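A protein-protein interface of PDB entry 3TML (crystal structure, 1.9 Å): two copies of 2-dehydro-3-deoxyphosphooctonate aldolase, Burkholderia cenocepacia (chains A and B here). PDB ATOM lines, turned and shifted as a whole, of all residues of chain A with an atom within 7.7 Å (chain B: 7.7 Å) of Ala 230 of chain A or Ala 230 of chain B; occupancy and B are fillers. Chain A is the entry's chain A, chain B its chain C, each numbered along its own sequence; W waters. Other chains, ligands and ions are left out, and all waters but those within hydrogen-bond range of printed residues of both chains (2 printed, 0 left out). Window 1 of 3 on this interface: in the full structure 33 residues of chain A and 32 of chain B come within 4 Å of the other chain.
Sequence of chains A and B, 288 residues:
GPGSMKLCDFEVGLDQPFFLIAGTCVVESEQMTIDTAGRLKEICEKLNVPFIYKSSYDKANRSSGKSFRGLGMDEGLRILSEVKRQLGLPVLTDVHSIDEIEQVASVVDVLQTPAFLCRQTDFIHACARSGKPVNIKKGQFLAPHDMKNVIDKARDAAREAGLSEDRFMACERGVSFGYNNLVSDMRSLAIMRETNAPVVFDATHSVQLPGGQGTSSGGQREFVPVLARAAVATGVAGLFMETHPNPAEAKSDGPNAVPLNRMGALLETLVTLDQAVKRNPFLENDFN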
ATOM      1  N   SER A 184       5.475 -25.843   9.480  1.00  0.00           N
ATOM      2  CA  SER A 184       6.032 -24.545   9.198  1.00  0.00           C
ATOM      3  C   SER A 184       6.192 -23.836  10.520  1.00  0.00           C
ATOM      4  O   SER A 184       5.209 -23.351  11.162  1.00  0.00           O
ATOM      5  CB  SER A 184       5.103 -23.814   8.217  1.00  0.00           C
ATOM      6  OG  SER A 184       5.649 -22.590   7.865  1.00  0.00           O
ATOM      7  N   MET A 186       7.163 -20.927  12.514  1.00  0.00           N
ATOM      8  CA  MET A 186       7.250 -19.508  12.300  1.00  0.00           C
ATOM      9  C   MET A 186       8.473 -18.940  12.999  1.00  0.00           C
ATOM     10  O   MET A 186       8.963 -17.919  12.560  1.00  0.00           O
ATOM     11  CB  MET A 186       5.992 -18.801  12.749  1.00  0.00           C
ATOM     12  CG  MET A 186       4.751 -19.221  11.960  1.00  0.00           C
ATOM     13  SD  MET A 186       4.888 -18.718  10.234  1.00  0.00           S
ATOM     14  CE  MET A 186       4.036 -19.995   9.316  1.00  0.00           C
ATOM     15  N   ARG A 187       8.998 -19.626  14.017  1.00  0.00           N
ATOM     16  CA  ARG A 187      10.229 -19.177  14.671  1.00  0.00           C
ATOM     17  C   ARG A 187      11.387 -19.142  13.694  1.00  0.00           C
ATOM     18  O   ARG A 187      12.311 -18.351  13.851  1.00  0.00           O
ATOM     19  CB  ARG A 187      10.631 -20.064  15.868  1.00  0.00           C
ATOM     20  CG  ARG A 187       9.627 -20.116  17.022  1.00  0.00           C
ATOM     21  CD  ARG A 187      10.088 -21.116  18.063  1.00  0.00           C
ATOM     22  NE  ARG A 187      10.058 -22.475  17.546  1.00  0.00           N
ATOM     23  CZ  ARG A 187      10.157 -23.595  18.262  1.00  0.00           C
ATOM     24  NH1 ARG A 187      10.333 -23.565  19.561  1.00  0.00           N
ATOM     25  NH2 ARG A 187      10.087 -24.779  17.653  1.00  0.00           N
ATOM     26  N   LEU A 189      11.522 -18.287  10.542  1.00  0.00           N
ATOM     27  CA  LEU A 189      11.533 -17.023   9.830  1.00  0.00           C
ATOM     28  C   LEU A 189      12.183 -15.888  10.597  1.00  0.00           C
ATOM     29  O   LEU A 189      12.748 -14.963   9.951  1.00  0.00           O
ATOM     30  CB  LEU A 189      10.126 -16.642   9.399  1.00  0.00           C
ATOM     31  CG  LEU A 189       9.344 -17.686   8.595  1.00  0.00           C
ATOM     32  CD1 LEU A 189       7.921 -17.170   8.389  1.00  0.00           C
ATOM     33  CD2 LEU A 189      10.045 -17.948   7.264  1.00  0.00           C
ATOM     34  N   PHE A 201       9.552 -17.005   2.314  1.00  0.00           N
ATOM     35  CA  PHE A 201       8.655 -18.097   2.692  1.00  0.00           C
ATOM     36  C   PHE A 201       8.036 -18.765   1.457  1.00  0.00           C
ATOM     37  O   PHE A 201       7.365 -18.128   0.681  1.00  0.00           O
ATOM     38  CB  PHE A 201       7.531 -17.561   3.582  1.00  0.00           C
ATOM     39  CG  PHE A 201       6.649 -18.620   4.131  1.00  0.00           C
ATOM     40  CD1 PHE A 201       7.159 -19.523   5.074  1.00  0.00           C
ATOM     41  CD2 PHE A 201       5.334 -18.741   3.705  1.00  0.00           C
ATOM     42  CE1 PHE A 201       6.396 -20.552   5.552  1.00  0.00           C
ATOM     43  CE2 PHE A 201       4.537 -19.756   4.187  1.00  0.00           C
ATOM     44  CZ  PHE A 201       5.077 -20.676   5.111  1.00  0.00           C
ATOM     45  N   VAL A 224      -2.600 -23.005   2.189  1.00  0.00           N
ATOM     46  CA  VAL A 224      -1.683 -22.052   1.561  1.00  0.00           C
ATOM     47  C   VAL A 224      -1.997 -20.625   2.047  1.00  0.00           C
ATOM     48  O   VAL A 224      -1.085 -19.946   2.504  1.00  0.00           O
ATOM     49  CB  VAL A 224      -1.588 -22.179   0.019  1.00  0.00           C
ATOM     50  CG1 VAL A 224      -0.643 -21.105  -0.589  1.00  0.00           C
ATOM     51  CG2 VAL A 224      -1.114 -23.580  -0.363  1.00  0.00           C
ATOM     52  N   PRO A 225      -3.263 -20.195   2.000  1.00  0.00           N
ATOM     53  CA  PRO A 225      -3.555 -18.834   2.518  1.00  0.00           C
ATOM     54  C   PRO A 225      -3.208 -18.735   4.008  1.00  0.00           C
ATOM     55  O   PRO A 225      -2.675 -17.721   4.470  1.00  0.00           O
ATOM     56  CB  PRO A 225      -5.064 -18.682   2.304  1.00  0.00           C
ATOM     57  CG  PRO A 225      -5.471 -19.727   1.337  1.00  0.00           C
ATOM     58  CD  PRO A 225      -4.465 -20.846   1.426  1.00  0.00           C
ATOM     59  N   VAL A 226      -3.476 -19.812   4.728  1.00  0.00           N
ATOM     60  CA  VAL A 226      -3.263 -19.843   6.162  1.00  0.00           C
ATOM     61  C   VAL A 226      -1.806 -19.588   6.448  1.00  0.00           C
ATOM     62  O   VAL A 226      -1.460 -18.686   7.232  1.00  0.00           O
ATOM     63  CB  VAL A 226      -3.691 -21.196   6.762  1.00  0.00           C
ATOM     64  CG1 VAL A 226      -3.113 -21.390   8.182  1.00  0.00           C
ATOM     65  CG2 VAL A 226      -5.205 -21.279   6.758  1.00  0.00           C
ATOM     66  N   LEU A 227      -0.919 -20.381   5.859  1.00  0.00           N
ATOM     67  CA  LEU A 227       0.516 -20.175   6.136  1.00  0.00           C
ATOM     68  C   LEU A 227       1.068 -18.850   5.563  1.00  0.00           C
ATOM     69  O   LEU A 227       1.938 -18.228   6.182  1.00  0.00           O
ATOM     70  CB  LEU A 227       1.358 -21.343   5.633  1.00  0.00           C
ATOM     71  CG  LEU A 227       1.048 -22.719   6.237  1.00  0.00           C
ATOM     72  CD1 LEU A 227       2.141 -23.688   5.815  1.00  0.00           C
ATOM     73  CD2 LEU A 227       0.881 -22.689   7.752  1.00  0.00           C
ATOM     74  N   ALA A 228       0.575 -18.428   4.395  1.00  0.00           N
ATOM     75  CA  ALA A 228       1.019 -17.146   3.787  1.00  0.00           C
ATOM     76  C   ALA A 228       0.737 -15.976   4.743  1.00  0.00           C
ATOM     77  O   ALA A 228       1.618 -15.142   4.984  1.00  0.00           O
ATOM     78  CB  ALA A 228       0.315 -16.881   2.453  1.00  0.00           C
ATOM     79  N   ARG A 229      -0.471 -15.928   5.268  1.00  0.00           N
ATOM     80  CA  ARG A 229      -0.878 -14.877   6.227  1.00  0.00           C
ATOM     81  C   ARG A 229       0.018 -14.941   7.461  1.00  0.00           C
ATOM     82  O   ARG A 229       0.579 -13.948   7.870  1.00  0.00           O
ATOM     83  CB  ARG A 229      -2.359 -14.977   6.628  1.00  0.00           C
ATOM     84  CG  ARG A 229      -3.383 -14.643   5.535  1.00  0.00           C
ATOM     85  CD  ARG A 229      -4.763 -14.352   6.090  1.00  0.00           C
ATOM     86  NE  ARG A 229      -5.254 -15.448   6.939  1.00  0.00           N
ATOM     87  CZ  ARG A 229      -5.910 -16.524   6.497  1.00  0.00           C
ATOM     88  NH1 ARG A 229      -6.196 -16.673   5.209  1.00  0.00           N
ATOM     89  NH2 ARG A 229      -6.283 -17.469   7.351  1.00  0.00           N
ATOM     90  N   ALA A 230       0.199 -16.138   8.020  1.00  0.00           N
ATOM     91  CA  ALA A 230       1.036 -16.288   9.219  1.00  0.00           C
ATOM     92  C   ALA A 230       2.484 -15.824   8.993  1.00  0.00           C
ATOM     93  O   ALA A 230       3.089 -15.170   9.869  1.00  0.00           O
ATOM     94  CB  ALA A 230       1.006 -17.747   9.714  1.00  0.00           C
ATOM     95  N   ALA A 231       3.079 -16.235   7.854  1.00  0.00           N
ATOM     96  CA  ALA A 231       4.474 -15.913   7.521  1.00  0.00           C
ATOM     97  C   ALA A 231       4.675 -14.422   7.297  1.00  0.00           C
ATOM     98  O   ALA A 231       5.651 -13.830   7.778  1.00  0.00           O
ATOM     99  CB  ALA A 231       4.909 -16.669   6.254  1.00  0.00           C
ATOM    100  N   VAL A 232       3.765 -13.811   6.543  1.00  0.00           N
ATOM    101  CA  VAL A 232       3.824 -12.343   6.310  1.00  0.00           C
ATOM    102  C   VAL A 232       3.682 -11.571   7.615  1.00  0.00           C
ATOM    103  O   VAL A 232       4.444 -10.638   7.851  1.00  0.00           O
ATOM    104  CB  VAL A 232       2.832 -11.882   5.215  1.00  0.00           C
ATOM    105  CG1 VAL A 232       2.771 -10.341   5.100  1.00  0.00           C
ATOM    106  CG2 VAL A 232       3.250 -12.493   3.865  1.00  0.00           C
ATOM    107  N   ALA A 233       2.764 -12.002   8.493  1.00  0.00           N
ATOM    108  CA  ALA A 233       2.590 -11.369   9.801  1.00  0.00           C
ATOM    109  C   ALA A 233       3.829 -11.578  10.699  1.00  0.00           C
ATOM    110  O   ALA A 233       4.201 -10.710  11.524  1.00  0.00           O
ATOM    111  CB  ALA A 233       1.319 -11.880  10.511  1.00  0.00           C
ATOM    112  N   THR A 234       4.483 -12.723  10.517  1.00  0.00           N
ATOM    113  CA  THR A 234       5.731 -12.993  11.195  1.00  0.00           C
ATOM    114  C   THR A 234       6.792 -12.015  10.767  1.00  0.00           C
ATOM    115  O   THR A 234       7.553 -11.520  11.607  1.00  0.00           O
ATOM    116  CB  THR A 234       6.207 -14.451  10.948  1.00  0.00           C
ATOM    117  OG1 THR A 234       5.255 -15.335  11.566  1.00  0.00           O
ATOM    118  CG2 THR A 234       7.597 -14.679  11.578  1.00  0.00           C
ATOM    119  N   GLY A 235       6.842 -11.733   9.467  1.00  0.00           N
ATOM    120  CA  GLY A 235       7.821 -10.771   8.942  1.00  0.00           C
ATOM    121  C   GLY A 235       8.881 -11.422   8.099  1.00  0.00           C
ATOM    122  O   GLY A 235       9.821 -12.058   8.618  1.00  0.00           O
ATOM    123  N   VAL A 236       8.680 -11.321   6.791  1.00  0.00           N
ATOM    124  CA  VAL A 236       9.587 -11.864   5.778  1.00  0.00           C
ATOM    125  C   VAL A 236       9.882 -10.825   4.691  1.00  0.00           C
ATOM    126  O   VAL A 236       9.195  -9.834   4.522  1.00  0.00           O
ATOM    127  CB  VAL A 236       8.982 -13.081   5.105  1.00  0.00           C
ATOM    128  CG1 VAL A 236       8.696 -14.200   6.140  1.00  0.00           C
ATOM    129  CG2 VAL A 236       7.691 -12.684   4.385  1.00  0.00           C
ATOM    130  N   LEU A 270      -2.449  -9.829   2.297  1.00  0.00           N
ATOM    131  CA  LEU A 270      -1.039  -9.898   2.655  1.00  0.00           C
ATOM    132  C   LEU A 270      -0.396  -8.540   2.716  1.00  0.00           C
ATOM    133  O   LEU A 270       0.384  -8.276   3.614  1.00  0.00           O
ATOM    134  CB  LEU A 270      -0.267 -10.840   1.718  1.00  0.00           C
ATOM    135  CG  LEU A 270      -0.764 -12.296   1.725  1.00  0.00           C
ATOM    136  CD1 LEU A 270       0.026 -13.162   0.727  1.00  0.00           C
ATOM    137  CD2 LEU A 270      -0.743 -12.879   3.136  1.00  0.00           C
ATOM    138  N   LEU A 273      -1.226  -6.882   6.046  1.00  0.00           N
ATOM    139  CA  LEU A 273      -0.474  -7.537   7.118  1.00  0.00           C
ATOM    140  C   LEU A 273       0.980  -7.099   7.100  1.00  0.00           C
ATOM    141  O   LEU A 273       1.558  -6.819   8.158  1.00  0.00           O
ATOM    142  CB  LEU A 273      -0.524  -9.069   6.970  1.00  0.00           C
ATOM    143  CG  LEU A 273      -1.887  -9.735   7.108  1.00  0.00           C
ATOM    144  CD1 LEU A 273      -1.811 -11.235   6.802  1.00  0.00           C
ATOM    145  CD2 LEU A 273      -2.434  -9.456   8.518  1.00  0.00           C
ATOM    146  N   VAL A 277       2.804  -5.017  10.206  1.00  0.00           N
ATOM    147  CA  VAL A 277       3.940  -5.485  11.022  1.00  0.00           C
ATOM    148  C   VAL A 277       5.255  -4.739  10.802  1.00  0.00           C
ATOM    149  O   VAL A 277       6.111  -4.718  11.669  1.00  0.00           O
ATOM    150  CB  VAL A 277       4.140  -7.025  10.913  1.00  0.00           C
ATOM    151  CG1 VAL A 277       2.816  -7.716  11.201  1.00  0.00           C
ATOM    152  CG2 VAL A 277       4.708  -7.427   9.545  1.00  0.00           C
ATOM    153  N   SER B 184       4.427 -24.680  16.880  1.00  0.00           N
ATOM    154  CA  SER B 184       3.117 -24.107  16.736  1.00  0.00           C
ATOM    155  C   SER B 184       2.707 -24.302  15.259  1.00  0.00           C
ATOM    156  O   SER B 184       3.191 -23.571  14.311  1.00  0.00           O
ATOM    157  CB  SER B 184       3.138 -22.618  17.190  1.00  0.00           C
ATOM    158  OG  SER B 184       1.827 -22.084  17.163  1.00  0.00           O
ATOM    159  N   MET B 186       0.358 -23.716  12.548  1.00  0.00           N
ATOM    160  CA  MET B 186      -0.720 -22.769  12.252  1.00  0.00           C
ATOM    161  C   MET B 186      -1.908 -23.446  11.573  1.00  0.00           C
ATOM    162  O   MET B 186      -3.045 -23.008  11.758  1.00  0.00           O
ATOM    163  CB  MET B 186      -0.211 -21.592  11.440  1.00  0.00           C
ATOM    164  CG  MET B 186       0.806 -20.742  12.188  1.00  0.00           C
ATOM    165  SD  MET B 186       0.212 -19.887  13.687  1.00  0.00           S
ATOM    166  CE  MET B 186       1.638 -19.931  14.778  1.00  0.00           C
ATOM    167  N   ARG B 187      -1.683 -24.573  10.914  1.00  0.00           N
ATOM    168  CA  ARG B 187      -2.789 -25.357  10.357  1.00  0.00           C
ATOM    169  C   ARG B 187      -3.810 -25.777  11.433  1.00  0.00           C
ATOM    170  O   ARG B 187      -4.971 -25.916  11.157  1.00  0.00           O
ATOM    171  CB  ARG B 187      -2.287 -26.627   9.663  1.00  0.00           C
ATOM    172  CG  ARG B 187      -1.434 -26.353   8.434  1.00  0.00           C
ATOM    173  CD  ARG B 187      -0.839 -27.612   7.846  1.00  0.00           C
ATOM    174  NE  ARG B 187      -0.018 -28.355   8.797  1.00  0.00           N
ATOM    175  CZ  ARG B 187       0.710 -29.429   8.489  1.00  0.00           C
ATOM    176  NH1 ARG B 187       0.702 -29.917   7.249  1.00  0.00           N
ATOM    177  NH2 ARG B 187       1.447 -30.040   9.417  1.00  0.00           N
ATOM    178  N   LEU B 189      -4.907 -24.184  14.026  1.00  0.00           N
ATOM    179  CA  LEU B 189      -5.826 -23.090  14.277  1.00  0.00           C
ATOM    180  C   LEU B 189      -6.985 -23.115  13.264  1.00  0.00           C
ATOM    181  O   LEU B 189      -8.116 -22.802  13.630  1.00  0.00           O
ATOM    182  CB  LEU B 189      -5.099 -21.745  14.267  1.00  0.00           C
ATOM    183  CG  LEU B 189      -4.007 -21.609  15.314  1.00  0.00           C
ATOM    184  CD1 LEU B 189      -3.341 -20.233  15.236  1.00  0.00           C
ATOM    185  CD2 LEU B 189      -4.580 -21.843  16.710  1.00  0.00           C
ATOM    186  N   PHE B 201      -5.508 -19.104  21.201  1.00  0.00           N
ATOM    187  CA  PHE B 201      -4.097 -19.387  21.007  1.00  0.00           C
ATOM    188  C   PHE B 201      -3.298 -18.999  22.233  1.00  0.00           C
ATOM    189  O   PHE B 201      -3.284 -17.841  22.611  1.00  0.00           O
ATOM    190  CB  PHE B 201      -3.545 -18.677  19.774  1.00  0.00           C
ATOM    191  CG  PHE B 201      -2.103 -19.001  19.484  1.00  0.00           C
ATOM    192  CD1 PHE B 201      -1.750 -20.271  19.050  1.00  0.00           C
ATOM    193  CD2 PHE B 201      -1.094 -18.059  19.668  1.00  0.00           C
ATOM    194  CE1 PHE B 201      -0.432 -20.604  18.832  1.00  0.00           C
ATOM    195  CE2 PHE B 201       0.244 -18.373  19.449  1.00  0.00           C
ATOM    196  CZ  PHE B 201       0.590 -19.649  19.025  1.00  0.00           C
ATOM    197  N   VAL B 224       7.403 -15.011  21.511  1.00  0.00           N
ATOM    198  CA  VAL B 224       6.001 -14.779  21.899  1.00  0.00           C
ATOM    199  C   VAL B 224       5.307 -13.800  20.933  1.00  0.00           C
ATOM    200  O   VAL B 224       4.252 -14.135  20.390  1.00  0.00           O
ATOM    201  CB  VAL B 224       5.904 -14.409  23.404  1.00  0.00           C
ATOM    202  CG1 VAL B 224       4.494 -14.012  23.809  1.00  0.00           C
ATOM    203  CG2 VAL B 224       6.360 -15.601  24.256  1.00  0.00           C
ATOM    204  N   PRO B 225       5.936 -12.638  20.633  1.00  0.00           N
ATOM    205  CA  PRO B 225       5.328 -11.735  19.627  1.00  0.00           C
ATOM    206  C   PRO B 225       5.230 -12.367  18.245  1.00  0.00           C
ATOM    207  O   PRO B 225       4.260 -12.119  17.533  1.00  0.00           O
ATOM    208  CB  PRO B 225       6.274 -10.524  19.571  1.00  0.00           C
ATOM    209  CG  PRO B 225       7.274 -10.693  20.673  1.00  0.00           C
ATOM    210  CD  PRO B 225       7.110 -12.047  21.312  1.00  0.00           C
ATOM    211  N   VAL B 226       6.243 -13.158  17.890  1.00  0.00           N
ATOM    212  CA  VAL B 226       6.303 -13.847  16.618  1.00  0.00           C
ATOM    213  C   VAL B 226       5.087 -14.741  16.510  1.00  0.00           C
ATOM    214  O   VAL B 226       4.263 -14.591  15.595  1.00  0.00           O
ATOM    215  CB  VAL B 226       7.600 -14.659  16.453  1.00  0.00           C
ATOM    216  CG1 VAL B 226       7.506 -15.619  15.237  1.00  0.00           C
ATOM    217  CG2 VAL B 226       8.816 -13.733  16.324  1.00  0.00           C
ATOM    218  N   LEU B 227       4.940 -15.663  17.458  1.00  0.00           N
ATOM    219  CA  LEU B 227       3.818 -16.570  17.369  1.00  0.00           C
ATOM    220  C   LEU B 227       2.464 -15.856  17.568  1.00  0.00           C
ATOM    221  O   LEU B 227       1.496 -16.283  16.966  1.00  0.00           O
ATOM    222  CB  LEU B 227       3.936 -17.721  18.365  1.00  0.00           C
ATOM    223  CG  LEU B 227       5.112 -18.710  18.221  1.00  0.00           C
ATOM    224  CD1 LEU B 227       4.887 -19.919  19.112  1.00  0.00           C
ATOM    225  CD2 LEU B 227       5.380 -19.140  16.801  1.00  0.00           C
ATOM    226  N   ALA B 228       2.372 -14.807  18.416  1.00  0.00           N
ATOM    227  CA  ALA B 228       1.090 -14.089  18.564  1.00  0.00           C
ATOM    228  C   ALA B 228       0.659 -13.449  17.213  1.00  0.00           C
ATOM    229  O   ALA B 228      -0.498 -13.581  16.775  1.00  0.00           O
ATOM    230  CB  ALA B 228       1.195 -13.023  19.680  1.00  0.00           C
ATOM    231  N   ARG B 229       1.595 -12.800  16.534  1.00  0.00           N
ATOM    232  CA  ARG B 229       1.265 -12.166  15.224  1.00  0.00           C
ATOM    233  C   ARG B 229       0.834 -13.212  14.179  1.00  0.00           C
ATOM    234  O   ARG B 229      -0.191 -13.023  13.479  1.00  0.00           O
ATOM    235  CB  ARG B 229       2.435 -11.355  14.659  1.00  0.00           C
ATOM    236  CG  ARG B 229       2.835 -10.125  15.472  1.00  0.00           C
ATOM    237  CD  ARG B 229       3.708  -9.214  14.619  1.00  0.00           C
ATOM    238  NE  ARG B 229       4.899  -9.934  14.148  1.00  0.00           N
ATOM    239  CZ  ARG B 229       6.055 -10.042  14.818  1.00  0.00           C
ATOM    240  NH1 ARG B 229       6.259  -9.403  15.969  1.00  0.00           N
ATOM    241  NH2 ARG B 229       7.052 -10.744  14.298  1.00  0.00           N
ATOM    242  N   ALA B 230       1.576 -14.323  14.098  1.00  0.00           N
ATOM    243  CA  ALA B 230       1.242 -15.419  13.188  1.00  0.00           C
ATOM    244  C   ALA B 230      -0.138 -15.991  13.432  1.00  0.00           C
ATOM    245  O   ALA B 230      -0.907 -16.200  12.495  1.00  0.00           O
ATOM    246  CB  ALA B 230       2.283 -16.543  13.265  1.00  0.00           C
ATOM    247  N   ALA B 231      -0.436 -16.263  14.691  1.00  0.00           N
ATOM    248  CA  ALA B 231      -1.739 -16.841  15.104  1.00  0.00           C
ATOM    249  C   ALA B 231      -2.905 -15.909  14.799  1.00  0.00           C
ATOM    250  O   ALA B 231      -3.952 -16.322  14.252  1.00  0.00           O
ATOM    251  CB  ALA B 231      -1.722 -17.135  16.607  1.00  0.00           C
ATOM    252  N   VAL B 232      -2.753 -14.646  15.172  1.00  0.00           N
ATOM    253  CA  VAL B 232      -3.855 -13.645  14.942  1.00  0.00           C
ATOM    254  C   VAL B 232      -4.078 -13.497  13.437  1.00  0.00           C
ATOM    255  O   VAL B 232      -5.243 -13.557  12.917  1.00  0.00           O
ATOM    256  CB  VAL B 232      -3.559 -12.293  15.682  1.00  0.00           C
ATOM    257  CG1 VAL B 232      -4.475 -11.169  15.199  1.00  0.00           C
ATOM    258  CG2 VAL B 232      -3.741 -12.507  17.182  1.00  0.00           C
ATOM    259  N   ALA B 233      -2.978 -13.440  12.676  1.00  0.00           N
ATOM    260  CA  ALA B 233      -3.102 -13.372  11.220  1.00  0.00           C
ATOM    261  C   ALA B 233      -3.701 -14.653  10.661  1.00  0.00           C
ATOM    262  O   ALA B 233      -4.421 -14.645   9.652  1.00  0.00           O
ATOM    263  CB  ALA B 233      -1.754 -13.128  10.570  1.00  0.00           C
ATOM    264  N   THR B 234      -3.385 -15.785  11.289  1.00  0.00           N
ATOM    265  CA  THR B 234      -4.011 -17.035  10.840  1.00  0.00           C
ATOM    266  C   THR B 234      -5.531 -16.949  11.036  1.00  0.00           C
ATOM    267  O   THR B 234      -6.330 -17.418  10.187  1.00  0.00           O
ATOM    268  CB  THR B 234      -3.449 -18.240  11.618  1.00  0.00           C
ATOM    269  OG1 THR B 234      -2.040 -18.354  11.287  1.00  0.00           O
ATOM    270  CG2 THR B 234      -4.244 -19.499  11.253  1.00  0.00           C
ATOM    271  N   GLY B 235      -5.905 -16.375  12.171  1.00  0.00           N
ATOM    272  CA  GLY B 235      -7.313 -16.185  12.522  1.00  0.00           C
ATOM    273  C   GLY B 235      -7.745 -17.016  13.703  1.00  0.00           C
ATOM    274  O   GLY B 235      -7.882 -18.228  13.614  1.00  0.00           O
ATOM    275  N   VAL B 236      -8.003 -16.339  14.818  1.00  0.00           N
ATOM    276  CA  VAL B 236      -8.428 -16.959  16.055  1.00  0.00           C
ATOM    277  C   VAL B 236      -9.501 -16.136  16.743  1.00  0.00           C
ATOM    278  O   VAL B 236      -9.742 -14.966  16.400  1.00  0.00           O
ATOM    279  CB  VAL B 236      -7.255 -17.152  17.057  1.00  0.00           C
ATOM    280  CG1 VAL B 236      -6.200 -18.124  16.499  1.00  0.00           C
ATOM    281  CG2 VAL B 236      -6.639 -15.819  17.434  1.00  0.00           C
ATOM    282  N   LEU B 270      -1.543  -6.463  17.132  1.00  0.00           N
ATOM    283  CA  LEU B 270      -2.435  -7.605  16.950  1.00  0.00           C
ATOM    284  C   LEU B 270      -3.855  -7.203  16.516  1.00  0.00           C
ATOM    285  O   LEU B 270      -4.420  -7.868  15.656  1.00  0.00           O
ATOM    286  CB  LEU B 270      -2.506  -8.478  18.200  1.00  0.00           C
ATOM    287  CG  LEU B 270      -1.195  -9.065  18.692  1.00  0.00           C
ATOM    288  CD1 LEU B 270      -1.361  -9.843  19.978  1.00  0.00           C
ATOM    289  CD2 LEU B 270      -0.536  -9.928  17.589  1.00  0.00           C
ATOM    290  N   LEU B 273      -3.839  -6.623  12.863  1.00  0.00           N
ATOM    291  CA  LEU B 273      -3.791  -7.886  12.129  1.00  0.00           C
ATOM    292  C   LEU B 273      -5.155  -8.574  12.131  1.00  0.00           C
ATOM    293  O   LEU B 273      -5.606  -9.049  11.102  1.00  0.00           O
ATOM    294  CB  LEU B 273      -2.727  -8.820  12.725  1.00  0.00           C
ATOM    295  CG  LEU B 273      -1.298  -8.263  12.769  1.00  0.00           C
ATOM    296  CD1 LEU B 273      -0.304  -9.210  13.449  1.00  0.00           C
ATOM    297  CD2 LEU B 273      -0.832  -7.918  11.347  1.00  0.00           C
ATOM    298  N   VAL B 277      -7.591  -9.504   8.710  1.00  0.00           N
ATOM    299  CA  VAL B 277      -7.912 -10.846   8.245  1.00  0.00           C
ATOM    300  C   VAL B 277      -9.392 -11.184   8.406  1.00  0.00           C
ATOM    301  O   VAL B 277      -9.925 -12.076   7.722  1.00  0.00           O
ATOM    302  CB  VAL B 277      -6.999 -11.924   8.884  1.00  0.00           C
ATOM    303  CG1 VAL B 277      -5.532 -11.571   8.608  1.00  0.00           C
ATOM    304  CG2 VAL B 277      -7.276 -12.121  10.394  1.00  0.00           C
HETATM  305  O   HOH W   1       5.050 -21.612  14.236  1.00  0.00           O
HETATM  306  O   HOH W   2       2.505 -23.483  10.781  1.00  0.00           O
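The backbone carbonyl oxygen of Ala 233 of chain A is in hydrogen-bond range of the guanidinium group of Arg 229 of chain B, 2.8 Å away. The backbone carbonyl oxygen of Thr 234 of chain B lies within hydrogen-bond range of the guanidinium group of Arg 229 of chain A (2.8 Å). NH2 of Arg 229 of chain B sits at hydrogen-bond distance from O of Thr 234 of chain A (2.8 Å). NE of Arg 229 of chain A is in hydrogen-bond range of O of Ala 233 of chain B.
The side-chain hydroxyl (OG1) of Thr 234 of chain B lies within hydrogen-bond range of the backbone carbonyl oxygen (O) of Ala 230 of chain B (2.7 Å).
Among the printed residues, pairs that only touch across the chains: Ser 184 of chain A with Ser 184 of chain B, Met 186 of chain A with Val 226 of chain B, Met 186 of chain A with Ala 230 of chain B, Val 226 of chain A with Met 186 of chain B, Val 226 of chain A with Thr 234 of chain B, Leu 227 of chain A with Met 186 of chain B, Arg 229 of chain A with Val 277 of chain B, Ala 230 of chain A with Met 186 of chain B, Ala 230 of chain A with Ala 230 of chain B, Ala 230 of chain A with Thr 234 of chain B, Ala 233 of chain A with Ala 233 of chain B, Thr 234 of chain A with Val 226 of chain B, Thr 234 of chain A with Ala 230 of chain B, Leu 273 of chain A with Leu 273 of chain B, Leu 273 of chain A with Val 277 of chain B, Val 277 of chain A with Arg 229 of chain B and Val 277 of chain A with Leu 273 of chain B.
Of chain B, only Met 186, Ala 230 and Thr 234 come within 4 Å of Ala 230 of chain A. Of chain A, only Met 186 (3.9 Å), Ala 230 (3.7 Å) and Thr 234 (3.6 Å) come within 4 Å of Ala 230 of chain B. Printed residues of chain A within 4 Å of Met 186 of chain B: Val 226, Leu 227 and Ala 230. Leu 189 of chain B touches none of the printed residues of chain A. Val 236 of chain B touches none of the printed residues of chain A. The nearest residue of chain B that does not touch Ala 230 of chain A is Ala 233 of chain B (4.4 Å).
Of the 21 printed residues of chain B, 9 touch a printed residue of chain A. Printed residues of chain B that touch a printed residue of chain A: Ser 184, Met 186, Val 226, Arg 229, Ala 230, Ala 233, Thr 234, Leu 273 and Val 277. Hydrophobic or aromatic side chains of chain B within 4 Å of the printed part of chain A: Met 186, Val 226, Ala 230, Ala 233, Leu 273 and Val 277.
Positions printed for both chains: 184, 186, 187, 189, 201, 224, 225, 226, 227, 228, 229, 230, 231, 232, 233, 234, 235, 236, 270, 273 and 277.
Water W1 bridges O of Ser 184 of chain B (2.7 Å) and N of Met 186 of chain A (2.8 Å). Water W2 lies within hydrogen-bond range of O of Ser 184 of chain A (2.7 Å) and N of Met 186 of chain B (2.8 Å).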
